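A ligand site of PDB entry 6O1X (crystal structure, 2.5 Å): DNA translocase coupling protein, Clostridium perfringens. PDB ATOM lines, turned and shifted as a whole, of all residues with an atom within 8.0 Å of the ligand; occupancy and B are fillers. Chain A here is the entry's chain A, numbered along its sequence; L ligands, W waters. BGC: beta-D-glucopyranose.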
ATOM      1  N   GLY A  39      17.992  17.449 -19.140  1.00  0.00           N
ATOM      2  CA  GLY A  39      17.474  18.706 -19.678  1.00  0.00           C
ATOM      3  C   GLY A  39      16.531  18.511 -20.855  1.00  0.00           C
ATOM      4  O   GLY A  39      15.413  19.045 -20.869  1.00  0.00           O
ATOM      5  N   VAL A 111       8.719  40.119 -19.762  1.00  0.00           N
ATOM      6  CA  VAL A 111       8.626  38.654 -19.736  1.00  0.00           C
ATOM      7  C   VAL A 111       7.909  38.112 -20.955  1.00  0.00           C
ATOM      8  O   VAL A 111       6.795  38.544 -21.264  1.00  0.00           O
ATOM      9  CB  VAL A 111       8.018  38.079 -18.413  1.00  0.00           C
ATOM     10  CG1 VAL A 111       8.155  36.563 -18.381  1.00  0.00           C
ATOM     11  CG2 VAL A 111       8.680  38.690 -17.187  1.00  0.00           C
ATOM     12  N   VAL A 112       8.538  37.124 -21.602  1.00  0.00           N
ATOM     13  CA  VAL A 112       7.911  36.438 -22.755  1.00  0.00           C
ATOM     14  C   VAL A 112       7.843  34.905 -22.540  1.00  0.00           C
ATOM     15  O   VAL A 112       8.653  34.353 -21.802  1.00  0.00           O
ATOM     16  CB  VAL A 112       8.483  36.809 -24.148  1.00  0.00           C
ATOM     17  CG1 VAL A 112       8.208  38.274 -24.462  1.00  0.00           C
ATOM     18  CG2 VAL A 112       9.968  36.464 -24.279  1.00  0.00           C
ATOM     19  N   VAL A 113       6.845  34.256 -23.168  1.00  0.00           N
ATOM     20  CA  VAL A 113       6.653  32.820 -23.123  1.00  0.00           C
ATOM     21  C   VAL A 113       6.835  32.274 -24.557  1.00  0.00           C
ATOM     22  O   VAL A 113       6.183  32.725 -25.500  1.00  0.00           O
ATOM     23  CB  VAL A 113       5.321  32.411 -22.465  1.00  0.00           C
ATOM     24  CG1 VAL A 113       5.374  30.953 -22.035  1.00  0.00           C
ATOM     25  CG2 VAL A 113       4.984  33.297 -21.262  1.00  0.00           C
ATOM     26  N   GLY A 115       7.026  28.750 -25.345  1.00  0.00           N
ATOM     27  CA  GLY A 115       6.449  27.421 -25.486  1.00  0.00           C
ATOM     28  C   GLY A 115       6.397  26.579 -24.234  1.00  0.00           C
ATOM     29  O   GLY A 115       6.608  27.072 -23.134  1.00  0.00           O
ATOM     30  N   GLN A 116       6.148  25.292 -24.422  1.00  0.00           N
ATOM     31  CA  GLN A 116       5.950  24.366 -23.316  1.00  0.00           C
ATOM     32  C   GLN A 116       7.007  23.314 -23.201  1.00  0.00           C
ATOM     33  O   GLN A 116       7.298  22.628 -24.174  1.00  0.00           O
ATOM     34  CB  GLN A 116       4.602  23.681 -23.497  1.00  0.00           C
ATOM     35  CG  GLN A 116       3.832  23.479 -22.217  1.00  0.00           C
ATOM     36  CD  GLN A 116       2.451  22.971 -22.537  1.00  0.00           C
ATOM     37  OE1 GLN A 116       2.224  21.759 -22.580  1.00  0.00           O
ATOM     38  NE2 GLN A 116       1.516  23.894 -22.787  1.00  0.00           N
ATOM     39  N   THR A 117       7.527  23.143 -21.998  1.00  0.00           N
ATOM     40  CA  THR A 117       8.457  22.036 -21.733  1.00  0.00           C
ATOM     41  C   THR A 117       7.688  20.942 -20.950  1.00  0.00           C
ATOM     42  O   THR A 117       6.464  20.972 -20.913  1.00  0.00           O
ATOM     43  CB  THR A 117       9.810  22.501 -21.130  1.00  0.00           C
ATOM     44  OG1 THR A 117      10.681  21.363 -21.054  1.00  0.00           O
ATOM     45  CG2 THR A 117       9.663  23.170 -19.772  1.00  0.00           C
ATOM     46  N   PHE A 118       8.416  19.971 -20.369  1.00  0.00           N
ATOM     47  CA  PHE A 118       7.876  18.820 -19.650  1.00  0.00           C
ATOM     48  C   PHE A 118       6.953  19.191 -18.494  1.00  0.00           C
ATOM     49  O   PHE A 118       5.904  18.580 -18.340  1.00  0.00           O
ATOM     50  CB  PHE A 118       9.027  17.907 -19.204  1.00  0.00           C
ATOM     51  CG  PHE A 118       9.821  17.421 -20.391  1.00  0.00           C
ATOM     52  CD1 PHE A 118       9.279  16.491 -21.277  1.00  0.00           C
ATOM     53  CD2 PHE A 118      11.072  17.962 -20.688  1.00  0.00           C
ATOM     54  CE1 PHE A 118       9.989  16.090 -22.404  1.00  0.00           C
ATOM     55  CE2 PHE A 118      11.788  17.535 -21.798  1.00  0.00           C
ATOM     56  CZ  PHE A 118      11.248  16.597 -22.652  1.00  0.00           C
ATOM     57  N   SER A 119       7.317  20.242 -17.737  1.00  0.00           N
ATOM     58  CA  SER A 119       6.520  20.758 -16.634  1.00  0.00           C
ATOM     59  C   SER A 119       6.550  22.281 -16.669  1.00  0.00           C
ATOM     60  O   SER A 119       7.471  22.904 -16.127  1.00  0.00           O
ATOM     61  CB  SER A 119       7.031  20.221 -15.307  1.00  0.00           C
ATOM     62  OG  SER A 119       6.298  20.753 -14.213  1.00  0.00           O
ATOM     63  N   GLY A 120       5.578  22.881 -17.336  1.00  0.00           N
ATOM     64  CA  GLY A 120       5.468  24.327 -17.435  1.00  0.00           C
ATOM     65  C   GLY A 120       5.986  24.913 -18.715  1.00  0.00           C
ATOM     66  O   GLY A 120       6.422  24.208 -19.637  1.00  0.00           O
ATOM     67  N   ASN A 121       5.916  26.226 -18.789  1.00  0.00           N
ATOM     68  CA  ASN A 121       6.336  26.989 -19.946  1.00  0.00           C
ATOM     69  C   ASN A 121       7.726  27.535 -19.851  1.00  0.00           C
ATOM     70  O   ASN A 121       8.251  27.692 -18.749  1.00  0.00           O
ATOM     71  CB  ASN A 121       5.348  28.098 -20.215  1.00  0.00           C
ATOM     72  CG  ASN A 121       3.965  27.610 -20.545  1.00  0.00           C
ATOM     73  OD1 ASN A 121       3.773  26.534 -21.119  1.00  0.00           O
ATOM     74  ND2 ASN A 121       2.968  28.407 -20.181  1.00  0.00           N
ATOM     75  N   ILE A 122       8.352  27.809 -21.009  1.00  0.00           N
ATOM     76  CA  ILE A 122       9.678  28.417 -21.067  1.00  0.00           C
ATOM     77  C   ILE A 122       9.411  29.913 -21.041  1.00  0.00           C
ATOM     78  O   ILE A 122       8.832  30.451 -21.969  1.00  0.00           O
ATOM     79  CB  ILE A 122      10.502  28.036 -22.340  1.00  0.00           C
ATOM     80  CG1 ILE A 122      10.734  26.514 -22.480  1.00  0.00           C
ATOM     81  CG2 ILE A 122      11.839  28.828 -22.376  1.00  0.00           C
ATOM     82  CD1 ILE A 122      11.687  25.806 -21.493  1.00  0.00           C
ATOM     83  N   LYS A 123       9.816  30.572 -19.974  1.00  0.00           N
ATOM     84  CA  LYS A 123       9.667  32.013 -19.822  1.00  0.00           C
ATOM     85  C   LYS A 123      11.022  32.646 -19.898  1.00  0.00           C
ATOM     86  O   LYS A 123      11.947  32.153 -19.288  1.00  0.00           O
ATOM     87  CB  LYS A 123       9.019  32.390 -18.484  1.00  0.00           C
ATOM     88  CG  LYS A 123       7.556  31.995 -18.392  1.00  0.00           C
ATOM     89  CD  LYS A 123       6.988  32.390 -17.055  1.00  0.00           C
ATOM     90  CE  LYS A 123       5.672  31.748 -16.774  1.00  0.00           C
ATOM     91  NZ  LYS A 123       5.072  32.333 -15.555  1.00  0.00           N
ATOM     92  N   ILE A 124      11.127  33.713 -20.670  1.00  0.00           N
ATOM     93  CA  ILE A 124      12.344  34.512 -20.776  1.00  0.00           C
ATOM     94  C   ILE A 124      12.043  35.912 -20.202  1.00  0.00           C
ATOM     95  O   ILE A 124      11.108  36.567 -20.665  1.00  0.00           O
ATOM     96  CB  ILE A 124      12.922  34.614 -22.226  1.00  0.00           C
ATOM     97  CG1 ILE A 124      13.006  33.228 -22.934  1.00  0.00           C
ATOM     98  CG2 ILE A 124      14.285  35.368 -22.222  1.00  0.00           C
ATOM     99  CD1 ILE A 124      13.224  33.318 -24.461  1.00  0.00           C
ATOM    100  N   ASP A 125      12.834  36.348 -19.202  1.00  0.00           N
ATOM    101  CA  ASP A 125      12.730  37.700 -18.645  1.00  0.00           C
ATOM    102  C   ASP A 125      13.839  38.533 -19.323  1.00  0.00           C
ATOM    103  O   ASP A 125      15.030  38.349 -19.058  1.00  0.00           O
ATOM    104  CB  ASP A 125      12.842  37.714 -17.105  1.00  0.00           C
ATOM    105  CG  ASP A 125      12.671  39.105 -16.466  1.00  0.00           C
ATOM    106  OD1 ASP A 125      12.550  40.112 -17.230  1.00  0.00           O
ATOM    107  OD2 ASP A 125      12.650  39.191 -15.206  1.00  0.00           O
ATOM    108  N   SER A 129      17.842  38.346 -19.246  1.00  0.00           N
ATOM    109  CA  SER A 129      18.459  37.726 -20.421  1.00  0.00           C
ATOM    110  C   SER A 129      18.074  38.589 -21.614  1.00  0.00           C
ATOM    111  O   SER A 129      16.995  38.375 -22.198  1.00  0.00           O
ATOM    112  CB  SER A 129      17.929  36.298 -20.577  1.00  0.00           C
ATOM    113  OG  SER A 129      18.157  35.506 -19.430  1.00  0.00           O
ATOM    114  N   VAL A 296      20.418  33.794 -24.582  1.00  0.00           N
ATOM    115  CA  VAL A 296      19.383  32.840 -24.947  1.00  0.00           C
ATOM    116  C   VAL A 296      19.603  32.277 -26.342  1.00  0.00           C
ATOM    117  O   VAL A 296      19.850  33.008 -27.314  1.00  0.00           O
ATOM    118  CB  VAL A 296      17.948  33.424 -24.750  1.00  0.00           C
ATOM    119  CG1 VAL A 296      16.866  32.495 -25.317  1.00  0.00           C
ATOM    120  CG2 VAL A 296      17.670  33.760 -23.275  1.00  0.00           C
ATOM    121  N   PHE A 329      16.123  24.822 -25.898  1.00  0.00           N
ATOM    122  CA  PHE A 329      16.252  26.088 -25.203  1.00  0.00           C
ATOM    123  C   PHE A 329      17.477  26.062 -24.359  1.00  0.00           C
ATOM    124  O   PHE A 329      17.587  25.196 -23.492  1.00  0.00           O
ATOM    125  CB  PHE A 329      15.037  26.375 -24.313  1.00  0.00           C
ATOM    126  CG  PHE A 329      15.166  27.638 -23.474  1.00  0.00           C
ATOM    127  CD1 PHE A 329      14.957  28.898 -24.044  1.00  0.00           C
ATOM    128  CD2 PHE A 329      15.461  27.562 -22.113  1.00  0.00           C
ATOM    129  CE1 PHE A 329      15.065  30.057 -23.267  1.00  0.00           C
ATOM    130  CE2 PHE A 329      15.546  28.722 -21.341  1.00  0.00           C
ATOM    131  CZ  PHE A 329      15.363  29.964 -21.920  1.00  0.00           C
ATOM    132  N   LYS A 330      18.369  27.023 -24.562  1.00  0.00           N
ATOM    133  CA  LYS A 330      19.580  27.133 -23.763  1.00  0.00           C
ATOM    134  C   LYS A 330      19.755  28.510 -23.117  1.00  0.00           C
ATOM    135  O   LYS A 330      19.713  29.526 -23.809  1.00  0.00           O
ATOM    136  CB  LYS A 330      20.837  26.711 -24.550  1.00  0.00           C
ATOM    137  CG  LYS A 330      22.113  26.739 -23.708  1.00  0.00           C
ATOM    138  CD  LYS A 330      23.267  27.432 -24.394  1.00  0.00           C
ATOM    139  CE  LYS A 330      24.472  27.539 -23.489  1.00  0.00           C
ATOM    140  NZ  LYS A 330      24.845  26.216 -22.911  1.00  0.00           N
ATOM    141  N   LEU A 331      19.957  28.508 -21.809  1.00  0.00           N
ATOM    142  CA  LEU A 331      20.252  29.708 -21.002  1.00  0.00           C
ATOM    143  C   LEU A 331      21.177  29.212 -19.915  1.00  0.00           C
ATOM    144  O   LEU A 331      20.780  28.364 -19.114  1.00  0.00           O
ATOM    145  CB  LEU A 331      18.972  30.374 -20.425  1.00  0.00           C
ATOM    146  CG  LEU A 331      19.221  31.635 -19.565  1.00  0.00           C
ATOM    147  CD1 LEU A 331      19.950  32.760 -20.349  1.00  0.00           C
ATOM    148  CD2 LEU A 331      17.957  32.114 -18.903  1.00  0.00           C
ATOM    149  N   GLY A 332      22.428  29.663 -19.952  1.00  0.00           N
ATOM    150  CA  GLY A 332      23.451  29.214 -19.024  1.00  0.00           C
ATOM    151  C   GLY A 332      23.679  27.718 -19.182  1.00  0.00           C
ATOM    152  O   GLY A 332      23.874  27.240 -20.299  1.00  0.00           O
ATOM    153  N   ALA A 333      23.571  26.968 -18.076  1.00  0.00           N
ATOM    154  CA  ALA A 333      23.743  25.500 -18.004  1.00  0.00           C
ATOM    155  C   ALA A 333      22.613  24.722 -18.619  1.00  0.00           C
ATOM    156  O   ALA A 333      22.766  23.523 -18.779  1.00  0.00           O
ATOM    157  CB  ALA A 333      23.887  25.058 -16.560  1.00  0.00           C
ATOM    158  N   ASP A 334      21.473  25.327 -18.888  1.00  0.00           N
ATOM    159  CA  ASP A 334      20.307  24.615 -19.384  1.00  0.00           C
ATOM    160  C   ASP A 334      20.235  24.419 -20.884  1.00  0.00           C
ATOM    161  O   ASP A 334      20.357  25.378 -21.615  1.00  0.00           O
ATOM    162  CB  ASP A 334      19.015  25.353 -18.971  1.00  0.00           C
ATOM    163  CG  ASP A 334      18.516  25.127 -17.556  1.00  0.00           C
ATOM    164  OD1 ASP A 334      19.175  24.362 -16.799  1.00  0.00           O
ATOM    165  OD2 ASP A 334      17.464  25.701 -17.203  1.00  0.00           O
ATOM    166  N   THR A 335      19.961  23.182 -21.329  1.00  0.00           N
ATOM    167  CA  THR A 335      19.634  22.803 -22.708  1.00  0.00           C
ATOM    168  C   THR A 335      18.381  21.941 -22.519  1.00  0.00           C
ATOM    169  O   THR A 335      18.486  20.785 -22.082  1.00  0.00           O
ATOM    170  CB  THR A 335      20.774  22.119 -23.460  1.00  0.00           C
ATOM    171  OG1 THR A 335      21.920  22.951 -23.394  1.00  0.00           O
ATOM    172  CG2 THR A 335      20.415  21.837 -24.910  1.00  0.00           C
ATOM    173  N   VAL A 336      17.206  22.559 -22.724  1.00  0.00           N
ATOM    174  CA  VAL A 336      15.887  21.996 -22.446  1.00  0.00           C
ATOM    175  C   VAL A 336      15.055  21.787 -23.716  1.00  0.00           C
ATOM    176  O   VAL A 336      15.015  22.658 -24.578  1.00  0.00           O
ATOM    177  CB  VAL A 336      15.155  22.883 -21.376  1.00  0.00           C
ATOM    178  CG1 VAL A 336      13.836  22.289 -20.950  1.00  0.00           C
ATOM    179  CG2 VAL A 336      16.030  23.106 -20.138  1.00  0.00           C
ATOM    180  N   GLN A 337      14.351  20.642 -23.822  1.00  0.00           N
ATOM    181  CA  GLN A 337      13.484  20.406 -24.968  1.00  0.00           C
ATOM    182  C   GLN A 337      12.126  21.092 -24.705  1.00  0.00           C
ATOM    183  O   GLN A 337      11.618  21.023 -23.588  1.00  0.00           O
ATOM    184  CB  GLN A 337      13.322  18.896 -25.219  1.00  0.00           C
ATOM    185  CG  GLN A 337      12.707  18.551 -26.558  1.00  0.00           C
ATOM    186  CD  GLN A 337      12.518  17.061 -26.823  1.00  0.00           C
ATOM    187  OE1 GLN A 337      11.652  16.678 -27.620  1.00  0.00           O
ATOM    188  NE2 GLN A 337      13.300  16.192 -26.181  1.00  0.00           N
ATOM    189  N   PHE A 338      11.559  21.769 -25.740  1.00  0.00           N
ATOM    190  CA  PHE A 338      10.260  22.440 -25.631  1.00  0.00           C
ATOM    191  C   PHE A 338       9.535  22.497 -26.954  1.00  0.00           C
ATOM    192  O   PHE A 338      10.154  22.463 -28.021  1.00  0.00           O
ATOM    193  CB  PHE A 338      10.376  23.853 -25.000  1.00  0.00           C
ATOM    194  CG  PHE A 338      10.853  24.941 -25.933  1.00  0.00           C
ATOM    195  CD1 PHE A 338      12.206  25.116 -26.200  1.00  0.00           C
ATOM    196  CD2 PHE A 338       9.942  25.818 -26.522  1.00  0.00           C
ATOM    197  CE1 PHE A 338      12.637  26.117 -27.065  1.00  0.00           C
ATOM    198  CE2 PHE A 338      10.385  26.826 -27.386  1.00  0.00           C
ATOM    199  CZ  PHE A 338      11.725  26.967 -27.649  1.00  0.00           C
HETATM  200  C2  BGC L   1      12.533  25.858 -17.307  1.00  0.00           C
HETATM  201  C3  BGC L   1      11.547  26.936 -17.707  1.00  0.00           C
HETATM  202  C4  BGC L   1      11.968  28.286 -17.120  1.00  0.00           C
HETATM  203  C5  BGC L   1      13.400  28.606 -17.566  1.00  0.00           C
HETATM  204  C6  BGC L   1      13.935  29.857 -16.901  1.00  0.00           C
HETATM  205  C1  BGC L   1      13.949  26.244 -17.708  1.00  0.00           C
HETATM  206  O1  BGC L   1      14.813  25.326 -17.162  1.00  0.00           O
HETATM  207  O2  BGC L   1      12.162  24.625 -17.912  1.00  0.00           O
HETATM  208  O3  BGC L   1      10.243  26.574 -17.261  1.00  0.00           O
HETATM  209  O4  BGC L   1      11.116  29.320 -17.579  1.00  0.00           O
HETATM  210  O5  BGC L   1      14.287  27.535 -17.190  1.00  0.00           O
HETATM  211  O6  BGC L   1      15.198  30.213 -17.430  1.00  0.00           O
HETATM  212  O   HOH W   1      14.676  32.231 -19.036  1.00  0.00           O
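N of Lys 123 sits at hydrogen-bond distance from O4 of the ligand (3.0 Å).
An oxygen (O4) of the ligand is in hydrogen-bond range of the backbone carbonyl oxygen (O) of Lys 123, at 3.4 Å.
O3 of the ligand is in hydrogen-bond range of O of Asn 121, at 2.7 Å.
OD2 of Asp 334 lies within hydrogen-bond range of O1 of the ligand, 2.7 Å away.
CG2 of Thr 117 touches O2 of the ligand, at 3.4 Å.
Ile 122 touches the ligand (CD1 to O2, 3.8 Å).
Leu 331 touches the ligand.
CG2 of Val 336 touches O1 of the ligand, at 3.9 Å.
Hydrophobic or aromatic side chains that line the ligand: Ile 122, Leu 331 and Val 336.
Within 4 Å of the ligand: Thr 117, Asn 121, Ile 122, Lys 123, Leu 331, Asp 334 and Val 336.
Water W1 bridges O6 of the ligand and O of Lys 123.
The backbone carbonyl oxygen (O) of Gln 337 sits at hydrogen-bond distance from the side-chain hydroxyl (OG1) of Thr 117.
N of Ile 122 lies within hydrogen-bond range of O of Gly 115 (2.8 Å).
O of Val 336 is in hydrogen-bond range of N of Phe 329, 2.8 Å away.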
